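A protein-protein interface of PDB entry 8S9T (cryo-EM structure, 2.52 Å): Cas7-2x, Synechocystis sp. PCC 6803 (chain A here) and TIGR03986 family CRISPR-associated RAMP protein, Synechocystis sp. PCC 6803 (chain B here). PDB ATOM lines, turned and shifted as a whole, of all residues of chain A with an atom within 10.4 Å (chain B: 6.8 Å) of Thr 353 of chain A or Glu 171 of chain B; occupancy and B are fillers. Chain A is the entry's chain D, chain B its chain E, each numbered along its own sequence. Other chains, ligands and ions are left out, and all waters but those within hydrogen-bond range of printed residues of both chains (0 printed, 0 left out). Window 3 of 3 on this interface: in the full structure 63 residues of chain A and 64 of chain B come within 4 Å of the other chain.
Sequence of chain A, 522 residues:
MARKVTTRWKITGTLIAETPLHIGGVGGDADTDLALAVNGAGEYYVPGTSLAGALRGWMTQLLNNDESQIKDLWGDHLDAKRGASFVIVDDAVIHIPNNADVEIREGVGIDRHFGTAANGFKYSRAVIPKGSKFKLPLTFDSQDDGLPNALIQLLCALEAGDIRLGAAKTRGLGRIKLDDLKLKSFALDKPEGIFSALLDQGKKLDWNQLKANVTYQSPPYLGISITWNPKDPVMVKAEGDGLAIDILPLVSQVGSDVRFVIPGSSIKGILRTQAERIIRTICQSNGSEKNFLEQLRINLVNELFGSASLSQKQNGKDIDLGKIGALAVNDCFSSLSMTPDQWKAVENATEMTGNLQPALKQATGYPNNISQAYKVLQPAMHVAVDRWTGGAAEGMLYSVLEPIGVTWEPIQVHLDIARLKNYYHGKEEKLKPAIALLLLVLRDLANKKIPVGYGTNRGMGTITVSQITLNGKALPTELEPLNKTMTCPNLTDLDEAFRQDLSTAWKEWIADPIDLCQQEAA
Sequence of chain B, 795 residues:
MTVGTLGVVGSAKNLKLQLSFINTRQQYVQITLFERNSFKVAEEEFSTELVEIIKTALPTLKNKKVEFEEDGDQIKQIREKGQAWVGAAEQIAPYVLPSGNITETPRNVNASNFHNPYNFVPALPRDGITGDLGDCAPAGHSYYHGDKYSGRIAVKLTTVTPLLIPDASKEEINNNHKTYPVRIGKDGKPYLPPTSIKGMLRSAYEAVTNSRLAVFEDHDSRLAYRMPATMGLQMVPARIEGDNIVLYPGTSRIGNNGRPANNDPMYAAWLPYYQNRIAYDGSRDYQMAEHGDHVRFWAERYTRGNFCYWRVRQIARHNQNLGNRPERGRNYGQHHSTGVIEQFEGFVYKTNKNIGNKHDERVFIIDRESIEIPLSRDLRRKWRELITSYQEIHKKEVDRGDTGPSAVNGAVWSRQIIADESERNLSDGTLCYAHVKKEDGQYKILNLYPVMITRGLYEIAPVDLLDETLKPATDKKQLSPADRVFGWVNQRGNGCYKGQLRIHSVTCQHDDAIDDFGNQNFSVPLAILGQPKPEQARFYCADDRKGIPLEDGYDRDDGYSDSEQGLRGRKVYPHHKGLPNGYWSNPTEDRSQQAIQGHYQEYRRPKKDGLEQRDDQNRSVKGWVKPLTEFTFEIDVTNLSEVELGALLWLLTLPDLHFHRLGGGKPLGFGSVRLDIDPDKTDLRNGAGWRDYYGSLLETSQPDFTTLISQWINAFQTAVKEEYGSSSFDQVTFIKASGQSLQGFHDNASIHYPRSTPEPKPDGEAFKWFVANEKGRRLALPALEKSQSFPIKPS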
ATOM      1  N   LEU A 243      -0.356   1.838 -32.480  1.00  0.00           N
ATOM      2  CA  LEU A 243       0.817   2.688 -32.396  1.00  0.00           C
ATOM      3  C   LEU A 243       1.767   2.224 -31.301  1.00  0.00           C
ATOM      4  O   LEU A 243       2.949   1.998 -31.563  1.00  0.00           O
ATOM      5  CB  LEU A 243       0.397   4.138 -32.156  1.00  0.00           C
ATOM      6  CG  LEU A 243      -0.156   4.914 -33.343  1.00  0.00           C
ATOM      7  CD1 LEU A 243      -0.862   6.146 -32.858  1.00  0.00           C
ATOM      8  CD2 LEU A 243       0.976   5.286 -34.268  1.00  0.00           C
ATOM      9  N   ALA A 244       1.271   2.072 -30.077  1.00  0.00           N
ATOM     10  CA  ALA A 244       2.093   1.463 -29.046  1.00  0.00           C
ATOM     11  C   ALA A 244       2.204  -0.045 -29.228  1.00  0.00           C
ATOM     12  O   ALA A 244       3.293  -0.605 -29.082  1.00  0.00           O
ATOM     13  CB  ALA A 244       1.530   1.787 -27.668  1.00  0.00           C
ATOM     14  N   ILE A 245       1.103  -0.717 -29.540  1.00  0.00           N
ATOM     15  CA  ILE A 245       1.069  -2.165 -29.686  1.00  0.00           C
ATOM     16  C   ILE A 245       0.960  -2.515 -31.160  1.00  0.00           C
ATOM     17  O   ILE A 245       0.064  -2.027 -31.847  1.00  0.00           O
ATOM     18  CB  ILE A 245      -0.093  -2.780 -28.894  1.00  0.00           C
ATOM     19  CG1 ILE A 245       0.027  -2.445 -27.416  1.00  0.00           C
ATOM     20  CG2 ILE A 245      -0.082  -4.255 -29.060  1.00  0.00           C
ATOM     21  CD1 ILE A 245       1.207  -3.067 -26.773  1.00  0.00           C
ATOM     22  N   ALA A 349      -3.234   4.891 -28.517  1.00  0.00           N
ATOM     23  CA  ALA A 349      -2.135   5.058 -27.579  1.00  0.00           C
ATOM     24  C   ALA A 349      -0.797   4.933 -28.291  1.00  0.00           C
ATOM     25  O   ALA A 349      -0.549   3.967 -29.014  1.00  0.00           O
ATOM     26  CB  ALA A 349      -2.243   4.027 -26.467  1.00  0.00           C
ATOM     27  N   THR A 350       0.045   5.944 -28.116  1.00  0.00           N
ATOM     28  CA  THR A 350       1.308   6.062 -28.827  1.00  0.00           C
ATOM     29  C   THR A 350       2.499   5.521 -28.052  1.00  0.00           C
ATOM     30  O   THR A 350       3.523   5.213 -28.665  1.00  0.00           O
ATOM     31  CB  THR A 350       1.566   7.528 -29.207  1.00  0.00           C
ATOM     32  OG1 THR A 350       1.847   8.295 -28.032  1.00  0.00           O
ATOM     33  CG2 THR A 350       0.363   8.121 -29.903  1.00  0.00           C
ATOM     34  N   GLU A 351       2.393   5.390 -26.736  1.00  0.00           N
ATOM     35  CA  GLU A 351       3.520   5.025 -25.892  1.00  0.00           C
ATOM     36  C   GLU A 351       3.112   3.931 -24.923  1.00  0.00           C
ATOM     37  O   GLU A 351       2.141   4.090 -24.182  1.00  0.00           O
ATOM     38  CB  GLU A 351       4.009   6.236 -25.101  1.00  0.00           C
ATOM     39  CG  GLU A 351       4.673   7.299 -25.921  1.00  0.00           C
ATOM     40  CD  GLU A 351       5.231   8.404 -25.060  1.00  0.00           C
ATOM     41  OE1 GLU A 351       6.356   8.877 -25.338  1.00  0.00           O
ATOM     42  OE2 GLU A 351       4.532   8.809 -24.107  1.00  0.00           O
ATOM     43  N   MET A 352       3.859   2.825 -24.934  1.00  0.00           N
ATOM     44  CA  MET A 352       3.465   1.657 -24.160  1.00  0.00           C
ATOM     45  C   MET A 352       3.455   1.947 -22.667  1.00  0.00           C
ATOM     46  O   MET A 352       2.568   1.483 -21.945  1.00  0.00           O
ATOM     47  CB  MET A 352       4.395   0.492 -24.473  1.00  0.00           C
ATOM     48  CG  MET A 352       4.205  -0.701 -23.563  1.00  0.00           C
ATOM     49  SD  MET A 352       5.281  -2.076 -23.952  1.00  0.00           S
ATOM     50  CE  MET A 352       4.461  -2.685 -25.410  1.00  0.00           C
ATOM     51  N   THR A 353       4.415   2.724 -22.186  1.00  0.00           N
ATOM     52  CA  THR A 353       4.425   3.157 -20.801  1.00  0.00           C
ATOM     53  C   THR A 353       3.945   4.583 -20.655  1.00  0.00           C
ATOM     54  O   THR A 353       3.940   5.118 -19.544  1.00  0.00           O
ATOM     55  CB  THR A 353       5.824   3.017 -20.190  1.00  0.00           C
ATOM     56  OG1 THR A 353       6.786   3.668 -21.025  1.00  0.00           O
ATOM     57  CG2 THR A 353       6.194   1.559 -20.029  1.00  0.00           C
ATOM     58  N   GLY A 354       3.533   5.200 -21.749  1.00  0.00           N
ATOM     59  CA  GLY A 354       2.857   6.468 -21.699  1.00  0.00           C
ATOM     60  C   GLY A 354       1.362   6.305 -21.690  1.00  0.00           C
ATOM     61  O   GLY A 354       0.807   5.643 -20.817  1.00  0.00           O
ATOM     62  N   ASN A 355       0.697   6.963 -22.630  1.00  0.00           N
ATOM     63  CA  ASN A 355      -0.754   7.050 -22.641  1.00  0.00           C
ATOM     64  C   ASN A 355      -1.458   5.711 -22.830  1.00  0.00           C
ATOM     65  O   ASN A 355      -2.679   5.661 -22.678  1.00  0.00           O
ATOM     66  CB  ASN A 355      -1.163   8.067 -23.699  1.00  0.00           C
ATOM     67  CG  ASN A 355      -0.527   7.804 -25.038  1.00  0.00           C
ATOM     68  OD1 ASN A 355      -0.348   6.668 -25.442  1.00  0.00           O
ATOM     69  ND2 ASN A 355      -0.150   8.866 -25.724  1.00  0.00           N
ATOM     70  N   LEU A 356      -0.734   4.632 -23.137  1.00  0.00           N
ATOM     71  CA  LEU A 356      -1.343   3.302 -23.145  1.00  0.00           C
ATOM     72  C   LEU A 356      -1.764   2.842 -21.758  1.00  0.00           C
ATOM     73  O   LEU A 356      -2.788   2.174 -21.611  1.00  0.00           O
ATOM     74  CB  LEU A 356      -0.381   2.288 -23.754  1.00  0.00           C
ATOM     75  CG  LEU A 356      -0.880   0.850 -23.884  1.00  0.00           C
ATOM     76  CD1 LEU A 356      -1.936   0.728 -24.960  1.00  0.00           C
ATOM     77  CD2 LEU A 356       0.264  -0.095 -24.152  1.00  0.00           C
ATOM     78  N   GLN A 357      -1.000   3.188 -20.728  1.00  0.00           N
ATOM     79  CA  GLN A 357      -1.359   2.735 -19.386  1.00  0.00           C
ATOM     80  C   GLN A 357      -2.666   3.331 -18.885  1.00  0.00           C
ATOM     81  O   GLN A 357      -3.476   2.580 -18.320  1.00  0.00           O
ATOM     82  CB  GLN A 357      -0.196   2.980 -18.423  1.00  0.00           C
ATOM     83  CG  GLN A 357       1.119   2.450 -18.917  1.00  0.00           C
ATOM     84  CD  GLN A 357       2.149   2.385 -17.825  1.00  0.00           C
ATOM     85  OE1 GLN A 357       2.068   3.115 -16.841  1.00  0.00           O
ATOM     86  NE2 GLN A 357       3.120   1.501 -17.978  1.00  0.00           N
ATOM     87  N   PRO A 358      -2.922   4.638 -18.996  1.00  0.00           N
ATOM     88  CA  PRO A 358      -4.293   5.124 -18.772  1.00  0.00           C
ATOM     89  C   PRO A 358      -5.343   4.403 -19.598  1.00  0.00           C
ATOM     90  O   PRO A 358      -6.382   3.998 -19.070  1.00  0.00           O
ATOM     91  CB  PRO A 358      -4.186   6.602 -19.148  1.00  0.00           C
ATOM     92  CG  PRO A 358      -2.825   6.943 -18.858  1.00  0.00           C
ATOM     93  CD  PRO A 358      -2.006   5.764 -19.234  1.00  0.00           C
ATOM     94  N   ALA A 359      -5.117   4.291 -20.903  1.00  0.00           N
ATOM     95  CA  ALA A 359      -6.098   3.695 -21.792  1.00  0.00           C
ATOM     96  C   ALA A 359      -6.407   2.251 -21.425  1.00  0.00           C
ATOM     97  O   ALA A 359      -7.560   1.822 -21.522  1.00  0.00           O
ATOM     98  CB  ALA A 359      -5.612   3.788 -23.235  1.00  0.00           C
ATOM     99  N   LEU A 360      -5.391   1.466 -21.056  1.00  0.00           N
ATOM    100  CA  LEU A 360      -5.647   0.090 -20.642  1.00  0.00           C
ATOM    101  C   LEU A 360      -6.298   0.010 -19.272  1.00  0.00           C
ATOM    102  O   LEU A 360      -7.140  -0.858 -19.036  1.00  0.00           O
ATOM    103  CB  LEU A 360      -4.368  -0.731 -20.664  1.00  0.00           C
ATOM    104  CG  LEU A 360      -3.812  -1.071 -22.035  1.00  0.00           C
ATOM    105  CD1 LEU A 360      -2.508  -1.788 -21.889  1.00  0.00           C
ATOM    106  CD2 LEU A 360      -4.794  -1.921 -22.795  1.00  0.00           C
ATOM    107  N   LYS A 361      -5.907   0.876 -18.350  1.00  0.00           N
ATOM    108  CA  LYS A 361      -6.590   0.942 -17.067  1.00  0.00           C
ATOM    109  C   LYS A 361      -8.075   1.239 -17.231  1.00  0.00           C
ATOM    110  O   LYS A 361      -8.911   0.629 -16.559  1.00  0.00           O
ATOM    111  CB  LYS A 361      -5.908   1.970 -16.171  1.00  0.00           C
ATOM    112  CG  LYS A 361      -4.640   1.431 -15.539  1.00  0.00           C
ATOM    113  CD  LYS A 361      -4.036   2.347 -14.505  1.00  0.00           C
ATOM    114  CE  LYS A 361      -3.654   3.662 -15.101  1.00  0.00           C
ATOM    115  NZ  LYS A 361      -3.013   4.532 -14.099  1.00  0.00           N
ATOM    116  N   ILE A 370      -2.950  -0.516 -11.988  1.00  0.00           N
ATOM    117  CA  ILE A 370      -2.278  -0.976 -13.197  1.00  0.00           C
ATOM    118  C   ILE A 370      -2.032  -2.478 -13.116  1.00  0.00           C
ATOM    119  O   ILE A 370      -2.010  -3.166 -14.140  1.00  0.00           O
ATOM    120  CB  ILE A 370      -0.979  -0.179 -13.437  1.00  0.00           C
ATOM    121  CG1 ILE A 370      -0.420  -0.451 -14.834  1.00  0.00           C
ATOM    122  CG2 ILE A 370       0.058  -0.498 -12.403  1.00  0.00           C
ATOM    123  CD1 ILE A 370      -1.333  -0.032 -15.949  1.00  0.00           C
ATOM    124  N   TYR A 374      -3.475  -4.995 -15.982  1.00  0.00           N
ATOM    125  CA  TYR A 374      -2.581  -5.849 -16.749  1.00  0.00           C
ATOM    126  C   TYR A 374      -2.754  -7.329 -16.449  1.00  0.00           C
ATOM    127  O   TYR A 374      -2.214  -8.154 -17.188  1.00  0.00           O
ATOM    128  CB  TYR A 374      -1.133  -5.426 -16.508  1.00  0.00           C
ATOM    129  CG  TYR A 374      -0.741  -4.214 -17.304  1.00  0.00           C
ATOM    130  CD1 TYR A 374      -1.701  -3.424 -17.903  1.00  0.00           C
ATOM    131  CD2 TYR A 374       0.581  -3.875 -17.487  1.00  0.00           C
ATOM    132  CE1 TYR A 374      -1.360  -2.327 -18.633  1.00  0.00           C
ATOM    133  CE2 TYR A 374       0.927  -2.782 -18.220  1.00  0.00           C
ATOM    134  CZ  TYR A 374      -0.047  -2.011 -18.790  1.00  0.00           C
ATOM    135  OH  TYR A 374       0.281  -0.907 -19.537  1.00  0.00           O
ATOM    136  N   PRO A 379       0.338  -5.995 -22.057  1.00  0.00           N
ATOM    137  CA  PRO A 379       1.264  -5.759 -23.167  1.00  0.00           C
ATOM    138  C   PRO A 379       2.504  -6.632 -23.033  1.00  0.00           C
ATOM    139  O   PRO A 379       3.070  -6.777 -21.951  1.00  0.00           O
ATOM    140  CB  PRO A 379       1.600  -4.271 -23.033  1.00  0.00           C
ATOM    141  CG  PRO A 379       0.626  -3.734 -22.070  1.00  0.00           C
ATOM    142  CD  PRO A 379       0.247  -4.830 -21.174  1.00  0.00           C
ATOM    143  N   ALA A 380       2.926  -7.213 -24.148  1.00  0.00           N
ATOM    144  CA  ALA A 380       4.049  -8.142 -24.171  1.00  0.00           C
ATOM    145  C   ALA A 380       4.990  -7.786 -25.306  1.00  0.00           C
ATOM    146  O   ALA A 380       4.565  -7.657 -26.454  1.00  0.00           O
ATOM    147  CB  ALA A 380       3.563  -9.580 -24.328  1.00  0.00           C
ATOM    148  N   MET A 381       6.266  -7.632 -24.984  1.00  0.00           N
ATOM    149  CA  MET A 381       7.308  -7.456 -25.982  1.00  0.00           C
ATOM    150  C   MET A 381       7.929  -8.783 -26.385  1.00  0.00           C
ATOM    151  O   MET A 381       8.112  -9.672 -25.557  1.00  0.00           O
ATOM    152  CB  MET A 381       8.382  -6.510 -25.460  1.00  0.00           C
ATOM    153  CG  MET A 381       7.957  -5.066 -25.498  1.00  0.00           C
ATOM    154  SD  MET A 381       7.868  -4.521 -27.207  1.00  0.00           S
ATOM    155  CE  MET A 381       8.268  -2.792 -27.030  1.00  0.00           C
ATOM    156  N   LEU A 397      11.818  -6.544 -33.314  1.00  0.00           N
ATOM    157  CA  LEU A 397      11.072  -6.307 -32.089  1.00  0.00           C
ATOM    158  C   LEU A 397       9.606  -6.021 -32.392  1.00  0.00           C
ATOM    159  O   LEU A 397       9.299  -5.175 -33.235  1.00  0.00           O
ATOM    160  CB  LEU A 397      11.707  -5.145 -31.334  1.00  0.00           C
ATOM    161  CG  LEU A 397      11.125  -4.609 -30.041  1.00  0.00           C
ATOM    162  CD1 LEU A 397      11.358  -5.589 -28.912  1.00  0.00           C
ATOM    163  CD2 LEU A 397      11.794  -3.306 -29.732  1.00  0.00           C
ATOM    164  N   SER A 399       5.369  -6.132 -30.483  1.00  0.00           N
ATOM    165  CA  SER A 399       4.609  -6.111 -29.244  1.00  0.00           C
ATOM    166  C   SER A 399       3.204  -6.646 -29.462  1.00  0.00           C
ATOM    167  O   SER A 399       2.616  -6.462 -30.527  1.00  0.00           O
ATOM    168  CB  SER A 399       4.548  -4.702 -28.654  1.00  0.00           C
ATOM    169  OG  SER A 399       3.856  -3.821 -29.502  1.00  0.00           O
ATOM    170  N   ASP B 167       8.950  -7.168 -17.021  1.00  0.00           N
ATOM    171  CA  ASP B 167       7.727  -6.627 -17.601  1.00  0.00           C
ATOM    172  C   ASP B 167       8.048  -5.260 -18.203  1.00  0.00           C
ATOM    173  O   ASP B 167       8.013  -4.237 -17.526  1.00  0.00           O
ATOM    174  CB  ASP B 167       6.606  -6.554 -16.580  1.00  0.00           C
ATOM    175  CG  ASP B 167       5.255  -6.544 -17.231  1.00  0.00           C
ATOM    176  OD1 ASP B 167       5.191  -6.351 -18.456  1.00  0.00           O
ATOM    177  OD2 ASP B 167       4.252  -6.742 -16.530  1.00  0.00           O
ATOM    178  N   ALA B 168       8.396  -5.255 -19.487  1.00  0.00           N
ATOM    179  CA  ALA B 168       8.654  -4.003 -20.181  1.00  0.00           C
ATOM    180  C   ALA B 168       7.417  -3.128 -20.254  1.00  0.00           C
ATOM    181  O   ALA B 168       7.540  -1.910 -20.412  1.00  0.00           O
ATOM    182  CB  ALA B 168       9.184  -4.271 -21.584  1.00  0.00           C
ATOM    183  N   SER B 169       6.229  -3.723 -20.168  1.00  0.00           N
ATOM    184  CA  SER B 169       4.990  -2.958 -20.144  1.00  0.00           C
ATOM    185  C   SER B 169       4.840  -2.109 -18.890  1.00  0.00           C
ATOM    186  O   SER B 169       4.006  -1.202 -18.870  1.00  0.00           O
ATOM    187  CB  SER B 169       3.803  -3.904 -20.289  1.00  0.00           C
ATOM    188  OG  SER B 169       3.536  -4.618 -19.102  1.00  0.00           O
ATOM    189  N   LYS B 170       5.616  -2.378 -17.848  1.00  0.00           N
ATOM    190  CA  LYS B 170       5.550  -1.619 -16.607  1.00  0.00           C
ATOM    191  C   LYS B 170       6.877  -0.965 -16.264  1.00  0.00           C
ATOM    192  O   LYS B 170       7.098  -0.609 -15.106  1.00  0.00           O
ATOM    193  CB  LYS B 170       5.116  -2.510 -15.448  1.00  0.00           C
ATOM    194  CG  LYS B 170       3.793  -3.180 -15.602  1.00  0.00           C
ATOM    195  CD  LYS B 170       3.451  -3.890 -14.319  1.00  0.00           C
ATOM    196  CE  LYS B 170       2.169  -4.669 -14.447  1.00  0.00           C
ATOM    197  NZ  LYS B 170       1.792  -5.360 -13.197  1.00  0.00           N
ATOM    198  N   GLU B 171       7.767  -0.807 -17.240  1.00  0.00           N
ATOM    199  CA  GLU B 171       9.080  -0.221 -17.010  1.00  0.00           C
ATOM    200  C   GLU B 171       9.001   1.215 -16.495  1.00  0.00           C
ATOM    201  O   GLU B 171       8.480   2.112 -17.161  1.00  0.00           O
ATOM    202  CB  GLU B 171       9.927  -0.319 -18.289  1.00  0.00           C
ATOM    203  CG  GLU B 171       9.519   0.608 -19.412  1.00  0.00           C
ATOM    204  CD  GLU B 171      10.192   0.315 -20.728  1.00  0.00           C
ATOM    205  OE1 GLU B 171      10.459  -0.865 -21.024  1.00  0.00           O
ATOM    206  OE2 GLU B 171      10.444   1.276 -21.480  1.00  0.00           O
ATOM    207  N   GLU B 172       9.444   1.421 -15.262  1.00  0.00           N
ATOM    208  CA  GLU B 172       9.656   2.758 -14.732  1.00  0.00           C
ATOM    209  C   GLU B 172      10.945   3.349 -15.291  1.00  0.00           C
ATOM    210  O   GLU B 172      11.969   2.672 -15.356  1.00  0.00           O
ATOM    211  CB  GLU B 172       9.725   2.696 -13.211  1.00  0.00           C
ATOM    212  CG  GLU B 172       8.467   3.159 -12.533  1.00  0.00           C
ATOM    213  CD  GLU B 172       7.387   2.096 -12.523  1.00  0.00           C
ATOM    214  OE1 GLU B 172       7.536   1.102 -11.785  1.00  0.00           O
ATOM    215  OE2 GLU B 172       6.385   2.253 -13.248  1.00  0.00           O
ATOM    216  N   ILE B 173      10.909   4.624 -15.674  1.00  0.00           N
ATOM    217  CA  ILE B 173      12.064   5.280 -16.285  1.00  0.00           C
ATOM    218  C   ILE B 173      12.370   6.558 -15.521  1.00  0.00           C
ATOM    219  O   ILE B 173      11.537   7.468 -15.465  1.00  0.00           O
ATOM    220  CB  ILE B 173      11.847   5.601 -17.771  1.00  0.00           C
ATOM    221  CG1 ILE B 173      11.053   4.496 -18.465  1.00  0.00           C
ATOM    222  CG2 ILE B 173      13.181   5.738 -18.455  1.00  0.00           C
ATOM    223  CD1 ILE B 173      10.863   4.722 -19.946  1.00  0.00           C
ATOM    224  N   LYS B 178      15.904   2.458 -16.754  1.00  0.00           N
ATOM    225  CA  LYS B 178      14.668   1.684 -16.737  1.00  0.00           C
ATOM    226  C   LYS B 178      14.685   0.668 -15.601  1.00  0.00           C
ATOM    227  O   LYS B 178      15.685  -0.019 -15.395  1.00  0.00           O
ATOM    228  CB  LYS B 178      14.470   0.972 -18.071  1.00  0.00           C
ATOM    229  CG  LYS B 178      14.379   1.904 -19.246  1.00  0.00           C
ATOM    230  CD  LYS B 178      14.124   1.162 -20.526  1.00  0.00           C
ATOM    231  CE  LYS B 178      13.957   2.117 -21.686  1.00  0.00           C
ATOM    232  NZ  LYS B 178      13.301   1.481 -22.864  1.00  0.00           N
ATOM    233  N   THR B 179      13.579   0.584 -14.866  1.00  0.00           N
ATOM    234  CA  THR B 179      13.395  -0.388 -13.795  1.00  0.00           C
ATOM    235  C   THR B 179      12.251  -1.316 -14.166  1.00  0.00           C
ATOM    236  O   THR B 179      11.148  -0.851 -14.457  1.00  0.00           O
ATOM    237  CB  THR B 179      13.108   0.300 -12.461  1.00  0.00           C
ATOM    238  OG1 THR B 179      14.168   1.205 -12.154  1.00  0.00           O
ATOM    239  CG2 THR B 179      13.002  -0.721 -11.355  1.00  0.00           C
ATOM    240  N   TYR B 180      12.514  -2.621 -14.168  1.00  0.00           N
ATOM    241  CA  TYR B 180      11.526  -3.595 -14.606  1.00  0.00           C
ATOM    242  C   TYR B 180      11.037  -4.429 -13.439  1.00  0.00           C
ATOM    243  O   TYR B 180      11.855  -4.990 -12.707  1.00  0.00           O
ATOM    244  CB  TYR B 180      12.110  -4.522 -15.667  1.00  0.00           C
ATOM    245  CG  TYR B 180      12.610  -3.841 -16.902  1.00  0.00           C
ATOM    246  CD1 TYR B 180      13.886  -3.310 -16.951  1.00  0.00           C
ATOM    247  CD2 TYR B 180      11.830  -3.764 -18.034  1.00  0.00           C
ATOM    248  CE1 TYR B 180      14.343  -2.678 -18.064  1.00  0.00           C
ATOM    249  CE2 TYR B 180      12.291  -3.154 -19.160  1.00  0.00           C
ATOM    250  CZ  TYR B 180      13.546  -2.606 -19.168  1.00  0.00           C
ATOM    251  OH  TYR B 180      14.017  -2.013 -20.309  1.00  0.00           O
ATOM    252  N   PRO B 181       9.732  -4.526 -13.225  1.00  0.00           N
ATOM    253  CA  PRO B 181       9.192  -5.564 -12.349  1.00  0.00           C
ATOM    254  C   PRO B 181       9.122  -6.905 -13.067  1.00  0.00           C
ATOM    255  O   PRO B 181       9.221  -6.992 -14.288  1.00  0.00           O
ATOM    256  CB  PRO B 181       7.807  -5.025 -12.018  1.00  0.00           C
ATOM    257  CG  PRO B 181       7.414  -4.323 -13.250  1.00  0.00           C
ATOM    258  CD  PRO B 181       8.656  -3.751 -13.861  1.00  0.00           C
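Printed residues of chain B that touch a printed residue of chain A: Ala 168, Ser 169, Lys 170 and Glu 171. Printed residues of chain A that touch a printed residue of chain B: Met 352, Thr 353, Gln 357, Tyr 374 and Pro 379. Hydrophobic or aromatic side chains of chain A within 4 Å of the printed part of chain B: Met 352, Tyr 374 and Pro 379. Among the printed residues, 8 pairs touch across the chains. Among the printed residues, no Asp or Glu carboxylate lies within 4 Å of a Lys or Arg side-chain nitrogen of the other chain.
The side-chain amide nitrogen (NE2) of Gln 357 of chain A is in hydrogen-bond range of the backbone carbonyl oxygen (O) of Ser 169 of chain B, at 3.0 Å.
The side-chain amino group (NZ) of Lys 178 of chain B lies within salt-bridge range of the side-chain carboxylate (OE2) of Glu 171 of chain B (3.2 Å). OG of Ser 169 of chain B is in hydrogen-bond range of OD1 of Asp 167 of chain B (2.5 Å).
Leu 243 of chain A touches none of the printed residues of chain B. Of chain B, only Ala 168 (3.7 Å), Ser 169 (3.7 Å) and Glu 171 (3.5 Å) come within 4 Å of Thr 353 of chain A. Printed residues of chain B within 4 Å of Gln 357 of chain A: Ser 169 (3.0 Å). Ala 168 of chain B touches just one residue of chain A: Thr 353. Of the printed residues of chain A, Lys 170 of chain B touches Tyr 374. Of the printed residues of chain A, Glu 171 of chain B touches Thr 353. No residue of chain A comes within 4 Å of Glu 172 of chain B. The nearest residue of chain A that does not touch Glu 171 of chain B is Gln 357 of chain A (5.2 Å).
Among the printed residues, merely in contact across the chains: Met 352 of chain A with Ser 169 of chain B, Thr 353 of chain A with Ala 168 of chain B, Thr 353 of chain A with Ser 169 of chain B, Thr 353 of chain A with Glu 171 of chain B, Tyr 374 of chain A with Ser 169 of chain B, Tyr 374 of chain A with Lys 170 of chain B and Pro 379 of chain A with Ser 169 of chain B.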
